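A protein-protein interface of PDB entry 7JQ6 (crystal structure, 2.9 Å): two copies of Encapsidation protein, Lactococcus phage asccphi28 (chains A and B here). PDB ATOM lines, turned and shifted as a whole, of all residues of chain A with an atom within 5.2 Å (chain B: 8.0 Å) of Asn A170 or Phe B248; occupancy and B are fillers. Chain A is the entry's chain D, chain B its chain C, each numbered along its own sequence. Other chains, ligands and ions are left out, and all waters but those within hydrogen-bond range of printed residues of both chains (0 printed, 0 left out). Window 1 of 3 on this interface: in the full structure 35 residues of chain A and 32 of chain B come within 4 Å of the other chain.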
ATOM      1  N   LYS A 133       0.747  39.944  24.461  1.00  0.00           N
ATOM      2  CA  LYS A 133       1.894  39.095  24.183  1.00  0.00           C
ATOM      3  C   LYS A 133       2.622  39.490  22.906  1.00  0.00           C
ATOM      4  O   LYS A 133       3.585  38.815  22.526  1.00  0.00           O
ATOM      5  CB  LYS A 133       1.466  37.625  24.094  1.00  0.00           C
ATOM      6  CG  LYS A 133       0.974  37.045  25.413  1.00  0.00           C
ATOM      7  CD  LYS A 133       2.062  37.071  26.481  1.00  0.00           C
ATOM      8  CE  LYS A 133       1.561  36.505  27.796  1.00  0.00           C
ATOM      9  NZ  LYS A 133       1.190  35.075  27.672  1.00  0.00           N
ATOM     10  N   THR A 166      -0.983  28.888  33.832  1.00  0.00           N
ATOM     11  CA  THR A 166      -0.920  28.883  32.375  1.00  0.00           C
ATOM     12  C   THR A 166      -0.541  30.255  31.825  1.00  0.00           C
ATOM     13  O   THR A 166       0.217  30.350  30.852  1.00  0.00           O
ATOM     14  CB  THR A 166      -2.261  28.424  31.800  1.00  0.00           C
ATOM     15  OG1 THR A 166      -2.512  27.072  32.203  1.00  0.00           O
ATOM     16  CG2 THR A 166      -2.241  28.500  30.283  1.00  0.00           C
ATOM     17  N   VAL A 167      -1.056  31.328  32.431  1.00  0.00           N
ATOM     18  CA  VAL A 167      -0.673  32.676  32.016  1.00  0.00           C
ATOM     19  C   VAL A 167       0.829  32.875  32.164  1.00  0.00           C
ATOM     20  O   VAL A 167       1.478  33.484  31.303  1.00  0.00           O
ATOM     21  CB  VAL A 167      -1.458  33.730  32.818  1.00  0.00           C
ATOM     22  CG1 VAL A 167      -0.963  35.131  32.477  1.00  0.00           C
ATOM     23  CG2 VAL A 167      -2.951  33.601  32.551  1.00  0.00           C
ATOM     24  N   LEU A 168       1.403  32.378  33.261  1.00  0.00           N
ATOM     25  CA  LEU A 168       2.839  32.521  33.482  1.00  0.00           C
ATOM     26  C   LEU A 168       3.632  31.791  32.404  1.00  0.00           C
ATOM     27  O   LEU A 168       4.574  32.348  31.830  1.00  0.00           O
ATOM     28  CB  LEU A 168       3.198  31.992  34.872  1.00  0.00           C
ATOM     29  CG  LEU A 168       4.658  32.072  35.322  1.00  0.00           C
ATOM     30  CD1 LEU A 168       5.137  33.509  35.324  1.00  0.00           C
ATOM     31  CD2 LEU A 168       4.830  31.457  36.701  1.00  0.00           C
ATOM     32  N   LEU A 169       3.244  30.549  32.097  1.00  0.00           N
ATOM     33  CA  LEU A 169       3.977  29.759  31.113  1.00  0.00           C
ATOM     34  C   LEU A 169       3.970  30.424  29.743  1.00  0.00           C
ATOM     35  O   LEU A 169       5.003  30.480  29.066  1.00  0.00           O
ATOM     36  CB  LEU A 169       3.377  28.357  31.021  1.00  0.00           C
ATOM     37  CG  LEU A 169       3.611  27.421  32.207  1.00  0.00           C
ATOM     38  CD1 LEU A 169       2.905  26.091  31.968  1.00  0.00           C
ATOM     39  CD2 LEU A 169       5.103  27.210  32.453  1.00  0.00           C
ATOM     40  N   ASN A 170       2.815  30.936  29.314  1.00  0.00           N
ATOM     41  CA  ASN A 170       2.758  31.662  28.050  1.00  0.00           C
ATOM     42  C   ASN A 170       3.684  32.873  28.076  1.00  0.00           C
ATOM     43  O   ASN A 170       4.319  33.202  27.066  1.00  0.00           O
ATOM     44  CB  ASN A 170       1.319  32.078  27.753  1.00  0.00           C
ATOM     45  CG  ASN A 170       0.430  30.896  27.397  1.00  0.00           C
ATOM     46  OD1 ASN A 170       0.897  29.888  26.861  1.00  0.00           O
ATOM     47  ND2 ASN A 170      -0.857  31.010  27.709  1.00  0.00           N
ATOM     48  N   LEU A 171       3.776  33.549  29.227  1.00  0.00           N
ATOM     49  CA  LEU A 171       4.681  34.688  29.354  1.00  0.00           C
ATOM     50  C   LEU A 171       6.135  34.251  29.230  1.00  0.00           C
ATOM     51  O   LEU A 171       6.967  35.001  28.704  1.00  0.00           O
ATOM     52  CB  LEU A 171       4.449  35.401  30.687  1.00  0.00           C
ATOM     53  CG  LEU A 171       5.380  36.581  30.975  1.00  0.00           C
ATOM     54  CD1 LEU A 171       5.371  37.585  29.833  1.00  0.00           C
ATOM     55  CD2 LEU A 171       4.994  37.268  32.280  1.00  0.00           C
ATOM     56  N   ILE A 172       6.463  33.056  29.719  1.00  0.00           N
ATOM     57  CA  ILE A 172       7.815  32.529  29.559  1.00  0.00           C
ATOM     58  C   ILE A 172       8.189  32.491  28.080  1.00  0.00           C
ATOM     59  O   ILE A 172       9.278  32.927  27.685  1.00  0.00           O
ATOM     60  CB  ILE A 172       7.928  31.135  30.203  1.00  0.00           C
ATOM     61  CG1 ILE A 172       7.599  31.190  31.699  1.00  0.00           C
ATOM     62  CG2 ILE A 172       9.324  30.560  29.993  1.00  0.00           C
ATOM     63  CD1 ILE A 172       8.552  32.024  32.520  1.00  0.00           C
ATOM     64  N   GLU A 173       7.290  31.972  27.238  1.00  0.00           N
ATOM     65  CA  GLU A 173       7.606  31.821  25.821  1.00  0.00           C
ATOM     66  C   GLU A 173       7.830  33.171  25.151  1.00  0.00           C
ATOM     67  O   GLU A 173       8.679  33.295  24.260  1.00  0.00           O
ATOM     68  CB  GLU A 173       6.488  31.060  25.109  1.00  0.00           C
ATOM     69  CG  GLU A 173       6.793  30.765  23.651  1.00  0.00           C
ATOM     70  CD  GLU A 173       5.684  29.995  22.968  1.00  0.00           C
ATOM     71  OE1 GLU A 173       4.729  29.589  23.661  1.00  0.00           O
ATOM     72  OE2 GLU A 173       5.768  29.794  21.739  1.00  0.00           O
ATOM     73  N   THR A 174       7.073  34.193  25.554  1.00  0.00           N
ATOM     74  CA  THR A 174       7.265  35.518  24.973  1.00  0.00           C
ATOM     75  C   THR A 174       8.596  36.108  25.422  1.00  0.00           C
ATOM     76  O   THR A 174       9.356  36.649  24.609  1.00  0.00           O
ATOM     77  CB  THR A 174       6.106  36.439  25.355  1.00  0.00           C
ATOM     78  OG1 THR A 174       4.891  35.942  24.781  1.00  0.00           O
ATOM     79  CG2 THR A 174       6.356  37.854  24.847  1.00  0.00           C
ATOM     80  N   ARG B  28      -0.282  30.788  16.727  1.00  0.00           N
ATOM     81  CA  ARG B  28       0.335  31.609  17.757  1.00  0.00           C
ATOM     82  C   ARG B  28       1.794  31.206  17.938  1.00  0.00           C
ATOM     83  O   ARG B  28       2.161  30.036  17.801  1.00  0.00           O
ATOM     84  CB  ARG B  28      -0.417  31.467  19.078  1.00  0.00           C
ATOM     85  CG  ARG B  28       0.156  32.314  20.200  1.00  0.00           C
ATOM     86  CD  ARG B  28      -0.567  32.065  21.506  1.00  0.00           C
ATOM     87  NE  ARG B  28      -1.935  32.574  21.483  1.00  0.00           N
ATOM     88  CZ  ARG B  28      -2.267  33.842  21.714  1.00  0.00           C
ATOM     89  NH1 ARG B  28      -1.328  34.741  21.982  1.00  0.00           N
ATOM     90  NH2 ARG B  28      -3.541  34.211  21.675  1.00  0.00           N
ATOM     91  N   ASP B 151      -9.707  36.294  22.750  1.00  0.00           N
ATOM     92  CA  ASP B 151      -9.392  34.956  23.236  1.00  0.00           C
ATOM     93  C   ASP B 151      -9.810  34.898  24.702  1.00  0.00           C
ATOM     94  O   ASP B 151      -9.290  35.656  25.529  1.00  0.00           O
ATOM     95  CB  ASP B 151      -7.905  34.653  23.065  1.00  0.00           C
ATOM     96  CG  ASP B 151      -7.549  33.234  23.454  1.00  0.00           C
ATOM     97  OD1 ASP B 151      -8.473  32.455  23.770  1.00  0.00           O
ATOM     98  OD2 ASP B 151      -6.346  32.895  23.433  1.00  0.00           O
ATOM     99  N   SER B 153      -9.359  32.715  27.110  1.00  0.00           N
ATOM    100  CA  SER B 153      -8.411  32.242  28.115  1.00  0.00           C
ATOM    101  C   SER B 153      -7.461  33.348  28.560  1.00  0.00           C
ATOM    102  O   SER B 153      -7.286  33.584  29.761  1.00  0.00           O
ATOM    103  CB  SER B 153      -7.623  31.053  27.563  1.00  0.00           C
ATOM    104  OG  SER B 153      -8.492  30.024  27.125  1.00  0.00           O
ATOM    105  N   ILE B 154      -6.837  34.037  27.605  1.00  0.00           N
ATOM    106  CA  ILE B 154      -5.829  35.039  27.940  1.00  0.00           C
ATOM    107  C   ILE B 154      -6.432  36.156  28.783  1.00  0.00           C
ATOM    108  O   ILE B 154      -5.856  36.572  29.795  1.00  0.00           O
ATOM    109  CB  ILE B 154      -5.174  35.583  26.655  1.00  0.00           C
ATOM    110  CG1 ILE B 154      -4.459  34.441  25.924  1.00  0.00           C
ATOM    111  CG2 ILE B 154      -4.217  36.727  26.977  1.00  0.00           C
ATOM    112  CD1 ILE B 154      -3.850  34.827  24.598  1.00  0.00           C
ATOM    113  N   PHE B 238      11.706  23.977  30.780  1.00  0.00           N
ATOM    114  CA  PHE B 238      10.454  24.697  30.576  1.00  0.00           C
ATOM    115  C   PHE B 238       9.511  23.919  29.669  1.00  0.00           C
ATOM    116  O   PHE B 238       8.298  23.879  29.904  1.00  0.00           O
ATOM    117  CB  PHE B 238      10.753  26.071  29.979  1.00  0.00           C
ATOM    118  CG  PHE B 238      11.718  26.889  30.793  1.00  0.00           C
ATOM    119  CD1 PHE B 238      11.843  26.696  32.160  1.00  0.00           C
ATOM    120  CD2 PHE B 238      12.524  27.831  30.184  1.00  0.00           C
ATOM    121  CE1 PHE B 238      12.738  27.441  32.900  1.00  0.00           C
ATOM    122  CE2 PHE B 238      13.420  28.571  30.921  1.00  0.00           C
ATOM    123  CZ  PHE B 238      13.526  28.379  32.280  1.00  0.00           C
ATOM    124  N   VAL B 239      10.054  23.294  28.625  1.00  0.00           N
ATOM    125  CA  VAL B 239       9.239  22.480  27.734  1.00  0.00           C
ATOM    126  C   VAL B 239       8.708  21.266  28.473  1.00  0.00           C
ATOM    127  O   VAL B 239       7.547  20.873  28.306  1.00  0.00           O
ATOM    128  CB  VAL B 239      10.053  22.075  26.494  1.00  0.00           C
ATOM    129  CG1 VAL B 239       9.276  21.084  25.645  1.00  0.00           C
ATOM    130  CG2 VAL B 239      10.420  23.303  25.678  1.00  0.00           C
ATOM    131  N   ARG B 240       9.555  20.644  29.294  1.00  0.00           N
ATOM    132  CA  ARG B 240       9.121  19.485  30.062  1.00  0.00           C
ATOM    133  C   ARG B 240       7.974  19.858  30.991  1.00  0.00           C
ATOM    134  O   ARG B 240       7.029  19.082  31.174  1.00  0.00           O
ATOM    135  CB  ARG B 240      10.294  18.917  30.860  1.00  0.00           C
ATOM    136  CG  ARG B 240      11.415  18.371  30.002  1.00  0.00           C
ATOM    137  CD  ARG B 240      12.523  17.717  30.827  1.00  0.00           C
ATOM    138  NE  ARG B 240      13.361  18.672  31.559  1.00  0.00           N
ATOM    139  CZ  ARG B 240      13.504  18.707  32.890  1.00  0.00           C
ATOM    140  NH1 ARG B 240      12.915  17.815  33.678  1.00  0.00           N
ATOM    141  NH2 ARG B 240      14.291  19.621  33.436  1.00  0.00           N
ATOM    142  N   LEU B 241       8.048  21.048  31.589  1.00  0.00           N
ATOM    143  CA  LEU B 241       7.020  21.503  32.518  1.00  0.00           C
ATOM    144  C   LEU B 241       5.696  21.765  31.811  1.00  0.00           C
ATOM    145  O   LEU B 241       4.626  21.444  32.343  1.00  0.00           O
ATOM    146  CB  LEU B 241       7.510  22.770  33.213  1.00  0.00           C
ATOM    147  CG  LEU B 241       6.690  23.317  34.374  1.00  0.00           C
ATOM    148  CD1 LEU B 241       6.699  22.341  35.540  1.00  0.00           C
ATOM    149  CD2 LEU B 241       7.225  24.677  34.783  1.00  0.00           C
ATOM    150  N   GLY B 242       5.745  22.363  30.618  1.00  0.00           N
ATOM    151  CA  GLY B 242       4.526  22.634  29.878  1.00  0.00           C
ATOM    152  C   GLY B 242       3.752  21.387  29.500  1.00  0.00           C
ATOM    153  O   GLY B 242       2.519  21.401  29.477  1.00  0.00           O
ATOM    154  N   ALA B 243       4.455  20.293  29.205  1.00  0.00           N
ATOM    155  CA  ALA B 243       3.771  19.062  28.828  1.00  0.00           C
ATOM    156  C   ALA B 243       2.914  18.538  29.973  1.00  0.00           C
ATOM    157  O   ALA B 243       1.828  17.992  29.745  1.00  0.00           O
ATOM    158  CB  ALA B 243       4.789  18.008  28.394  1.00  0.00           C
ATOM    159  N   LYS B 244       3.389  18.691  31.211  1.00  0.00           N
ATOM    160  CA  LYS B 244       2.642  18.191  32.361  1.00  0.00           C
ATOM    161  C   LYS B 244       1.324  18.936  32.552  1.00  0.00           C
ATOM    162  O   LYS B 244       0.341  18.343  33.011  1.00  0.00           O
ATOM    163  CB  LYS B 244       3.496  18.317  33.623  1.00  0.00           C
ATOM    164  CG  LYS B 244       4.743  17.446  33.621  1.00  0.00           C
ATOM    165  CD  LYS B 244       5.562  17.657  34.885  1.00  0.00           C
ATOM    166  CE  LYS B 244       6.886  16.910  34.828  1.00  0.00           C
ATOM    167  NZ  LYS B 244       7.775  17.269  35.970  1.00  0.00           N
ATOM    168  N   ASN B 245       1.284  20.223  32.211  1.00  0.00           N
ATOM    169  CA  ASN B 245       0.079  21.041  32.323  1.00  0.00           C
ATOM    170  C   ASN B 245      -0.625  21.061  30.971  1.00  0.00           C
ATOM    171  O   ASN B 245      -0.102  21.615  29.998  1.00  0.00           O
ATOM    172  CB  ASN B 245       0.425  22.452  32.790  1.00  0.00           C
ATOM    173  CG  ASN B 245       0.961  22.476  34.205  1.00  0.00           C
ATOM    174  OD1 ASN B 245       2.107  22.854  34.442  1.00  0.00           O
ATOM    175  ND2 ASN B 245       0.131  22.062  35.156  1.00  0.00           N
ATOM    176  N   ARG B 246      -1.820  20.466  30.917  1.00  0.00           N
ATOM    177  CA  ARG B 246      -2.503  20.281  29.642  1.00  0.00           C
ATOM    178  C   ARG B 246      -3.060  21.591  29.100  1.00  0.00           C
ATOM    179  O   ARG B 246      -3.009  21.838  27.889  1.00  0.00           O
ATOM    180  CB  ARG B 246      -3.635  19.272  29.813  1.00  0.00           C
ATOM    181  CG  ARG B 246      -3.174  17.872  30.141  1.00  0.00           C
ATOM    182  CD  ARG B 246      -2.627  17.163  28.915  1.00  0.00           C
ATOM    183  NE  ARG B 246      -3.634  17.032  27.865  1.00  0.00           N
ATOM    184  CZ  ARG B 246      -3.420  16.442  26.693  1.00  0.00           C
ATOM    185  NH1 ARG B 246      -2.231  15.923  26.416  1.00  0.00           N
ATOM    186  NH2 ARG B 246      -4.394  16.375  25.798  1.00  0.00           N
ATOM    187  N   ASP B 247      -3.612  22.432  29.975  1.00  0.00           N
ATOM    188  CA  ASP B 247      -4.174  23.702  29.527  1.00  0.00           C
ATOM    189  C   ASP B 247      -3.140  24.536  28.781  1.00  0.00           C
ATOM    190  O   ASP B 247      -3.486  25.258  27.838  1.00  0.00           O
ATOM    191  CB  ASP B 247      -4.729  24.469  30.730  1.00  0.00           C
ATOM    192  CG  ASP B 247      -5.444  25.745  30.333  1.00  0.00           C
ATOM    193  OD1 ASP B 247      -6.549  25.651  29.758  1.00  0.00           O
ATOM    194  OD2 ASP B 247      -4.913  26.840  30.605  1.00  0.00           O
ATOM    195  N   PHE B 248      -1.868  24.450  29.183  1.00  0.00           N
ATOM    196  CA  PHE B 248      -0.810  25.176  28.488  1.00  0.00           C
ATOM    197  C   PHE B 248      -0.512  24.571  27.120  1.00  0.00           C
ATOM    198  O   PHE B 248      -0.339  25.304  26.139  1.00  0.00           O
ATOM    199  CB  PHE B 248       0.454  25.208  29.350  1.00  0.00           C
ATOM    200  CG  PHE B 248       1.639  25.831  28.667  1.00  0.00           C
ATOM    201  CD1 PHE B 248       1.634  27.177  28.339  1.00  0.00           C
ATOM    202  CD2 PHE B 248       2.766  25.081  28.376  1.00  0.00           C
ATOM    203  CE1 PHE B 248       2.721  27.757  27.713  1.00  0.00           C
ATOM    204  CE2 PHE B 248       3.858  25.657  27.754  1.00  0.00           C
ATOM    205  CZ  PHE B 248       3.835  26.997  27.425  1.00  0.00           C
ATOM    206  N   SER B 249      -0.446  23.239  27.031  1.00  0.00           N
ATOM    207  CA  SER B 249      -0.087  22.600  25.769  1.00  0.00           C
ATOM    208  C   SER B 249      -1.128  22.884  24.694  1.00  0.00           C
ATOM    209  O   SER B 249      -0.786  23.138  23.534  1.00  0.00           O
ATOM    210  CB  SER B 249       0.076  21.092  25.968  1.00  0.00           C
ATOM    211  OG  SER B 249       1.032  20.805  26.974  1.00  0.00           O
ATOM    212  N   ASN B 250      -2.408  22.837  25.063  1.00  0.00           N
ATOM    213  CA  ASN B 250      -3.477  23.080  24.106  1.00  0.00           C
ATOM    214  C   ASN B 250      -3.459  24.505  23.565  1.00  0.00           C
ATOM    215  O   ASN B 250      -4.032  24.756  22.500  1.00  0.00           O
ATOM    216  CB  ASN B 250      -4.833  22.803  24.759  1.00  0.00           C
ATOM    217  CG  ASN B 250      -4.971  21.369  25.227  1.00  0.00           C
ATOM    218  OD1 ASN B 250      -4.131  20.522  24.927  1.00  0.00           O
ATOM    219  ND2 ASN B 250      -6.037  21.088  25.966  1.00  0.00           N
ATOM    220  N   SER B 251      -2.811  25.442  24.268  1.00  0.00           N
ATOM    221  CA  SER B 251      -2.867  26.841  23.855  1.00  0.00           C
ATOM    222  C   SER B 251      -2.297  27.053  22.458  1.00  0.00           C
ATOM    223  O   SER B 251      -2.791  27.909  21.713  1.00  0.00           O
ATOM    224  CB  SER B 251      -2.111  27.708  24.867  1.00  0.00           C
ATOM    225  OG  SER B 251      -2.162  29.077  24.507  1.00  0.00           O
ATOM    226  N   LYS B 252      -1.273  26.290  22.074  1.00  0.00           N
ATOM    227  CA  LYS B 252      -0.702  26.479  20.744  1.00  0.00           C
ATOM    228  C   LYS B 252      -1.691  26.066  19.662  1.00  0.00           C
ATOM    229  O   LYS B 252      -1.791  26.727  18.622  1.00  0.00           O
ATOM    230  CB  LYS B 252       0.620  25.729  20.602  1.00  0.00           C
ATOM    231  CG  LYS B 252       1.738  26.300  21.460  1.00  0.00           C
ATOM    232  CD  LYS B 252       3.057  25.604  21.171  1.00  0.00           C
ATOM    233  CE  LYS B 252       4.189  26.204  21.982  1.00  0.00           C
ATOM    234  NZ  LYS B 252       4.497  27.584  21.510  1.00  0.00           N
ATOM    235  N   THR B 253      -2.425  24.977  19.884  1.00  0.00           N
ATOM    236  CA  THR B 253      -3.440  24.527  18.943  1.00  0.00           C
ATOM    237  C   THR B 253      -4.840  24.929  19.391  1.00  0.00           C
ATOM    238  O   THR B 253      -5.827  24.412  18.858  1.00  0.00           O
ATOM    239  CB  THR B 253      -3.368  23.009  18.764  1.00  0.00           C
ATOM    240  OG1 THR B 253      -3.543  22.364  20.033  1.00  0.00           O
ATOM    241  CG2 THR B 253      -2.029  22.602  18.167  1.00  0.00           C
ATOM    242  N   ASN B 254      -4.941  25.843  20.361  1.00  0.00           N
ATOM    243  CA  ASN B 254      -6.234  26.280  20.870  1.00  0.00           C
ATOM    244  C   ASN B 254      -7.003  27.092  19.839  1.00  0.00           C
ATOM    245  O   ASN B 254      -8.233  27.180  19.926  1.00  0.00           O
ATOM    246  CB  ASN B 254      -6.035  27.104  22.145  1.00  0.00           C
ATOM    247  CG  ASN B 254      -7.328  27.692  22.669  1.00  0.00           C
ATOM    248  OD1 ASN B 254      -8.401  27.110  22.508  1.00  0.00           O
ATOM    249  ND2 ASN B 254      -7.233  28.856  23.301  1.00  0.00           N
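OD2 of Asp B247 is in hydrogen-bond range of OG1 of Thr A166, at 2.9 Å.
The side-chain amino group (NZ) of Lys B252 lies within salt-bridge range of the side-chain carboxylate (OE2) of Glu A173, at 2.6 Å.
The backbone carbonyl oxygen of Thr A166 is in hydrogen-bond range of the side-chain amide nitrogen of Asn A170 (3.4 Å).
Among the printed residues, merely in contact across the chains: Asn A170 with Phe B248 (2.9 Å), Leu A169 with Phe B248 (3.4 Å) and Asn A170 with Ser B251 (3.9 Å).
Asn A170 touches two residues of chain B.
Phe B248 touches two residues of chain A.
Of the printed residues of chain B, Glu A173 touches Lys B252.
Printed residues of chain A within 4 Å of Lys B252: Glu A173.
Of the printed residues of chain A, Asp B247 touches Thr A166 (2.9 Å).
Of the printed residues of chain A, Ser B251 touches Asn A170.
Printed residues of chain B within 4 Å of Leu A169: Phe B248.
Thr B253 touches none of the printed residues of chain A.
Of the 10 printed residues of chain A, 4 touch a printed residue of chain B.
Hydrophobic or aromatic side chains of chain A that line the printed part of chain B: Leu A169.
Along chain A the printed residues that touch a printed residue of chain B span positions 166 to 173.
Hydrophobic or aromatic side chains of chain B within 4 Å of the printed part of chain A: Phe B248.
Among the printed residues, 5 pairs touch across the chains.
No position is printed for both chains.
Of the 5 pairs that touch across the chains among the printed residues, none has its exchanged pair printed and touching as well.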
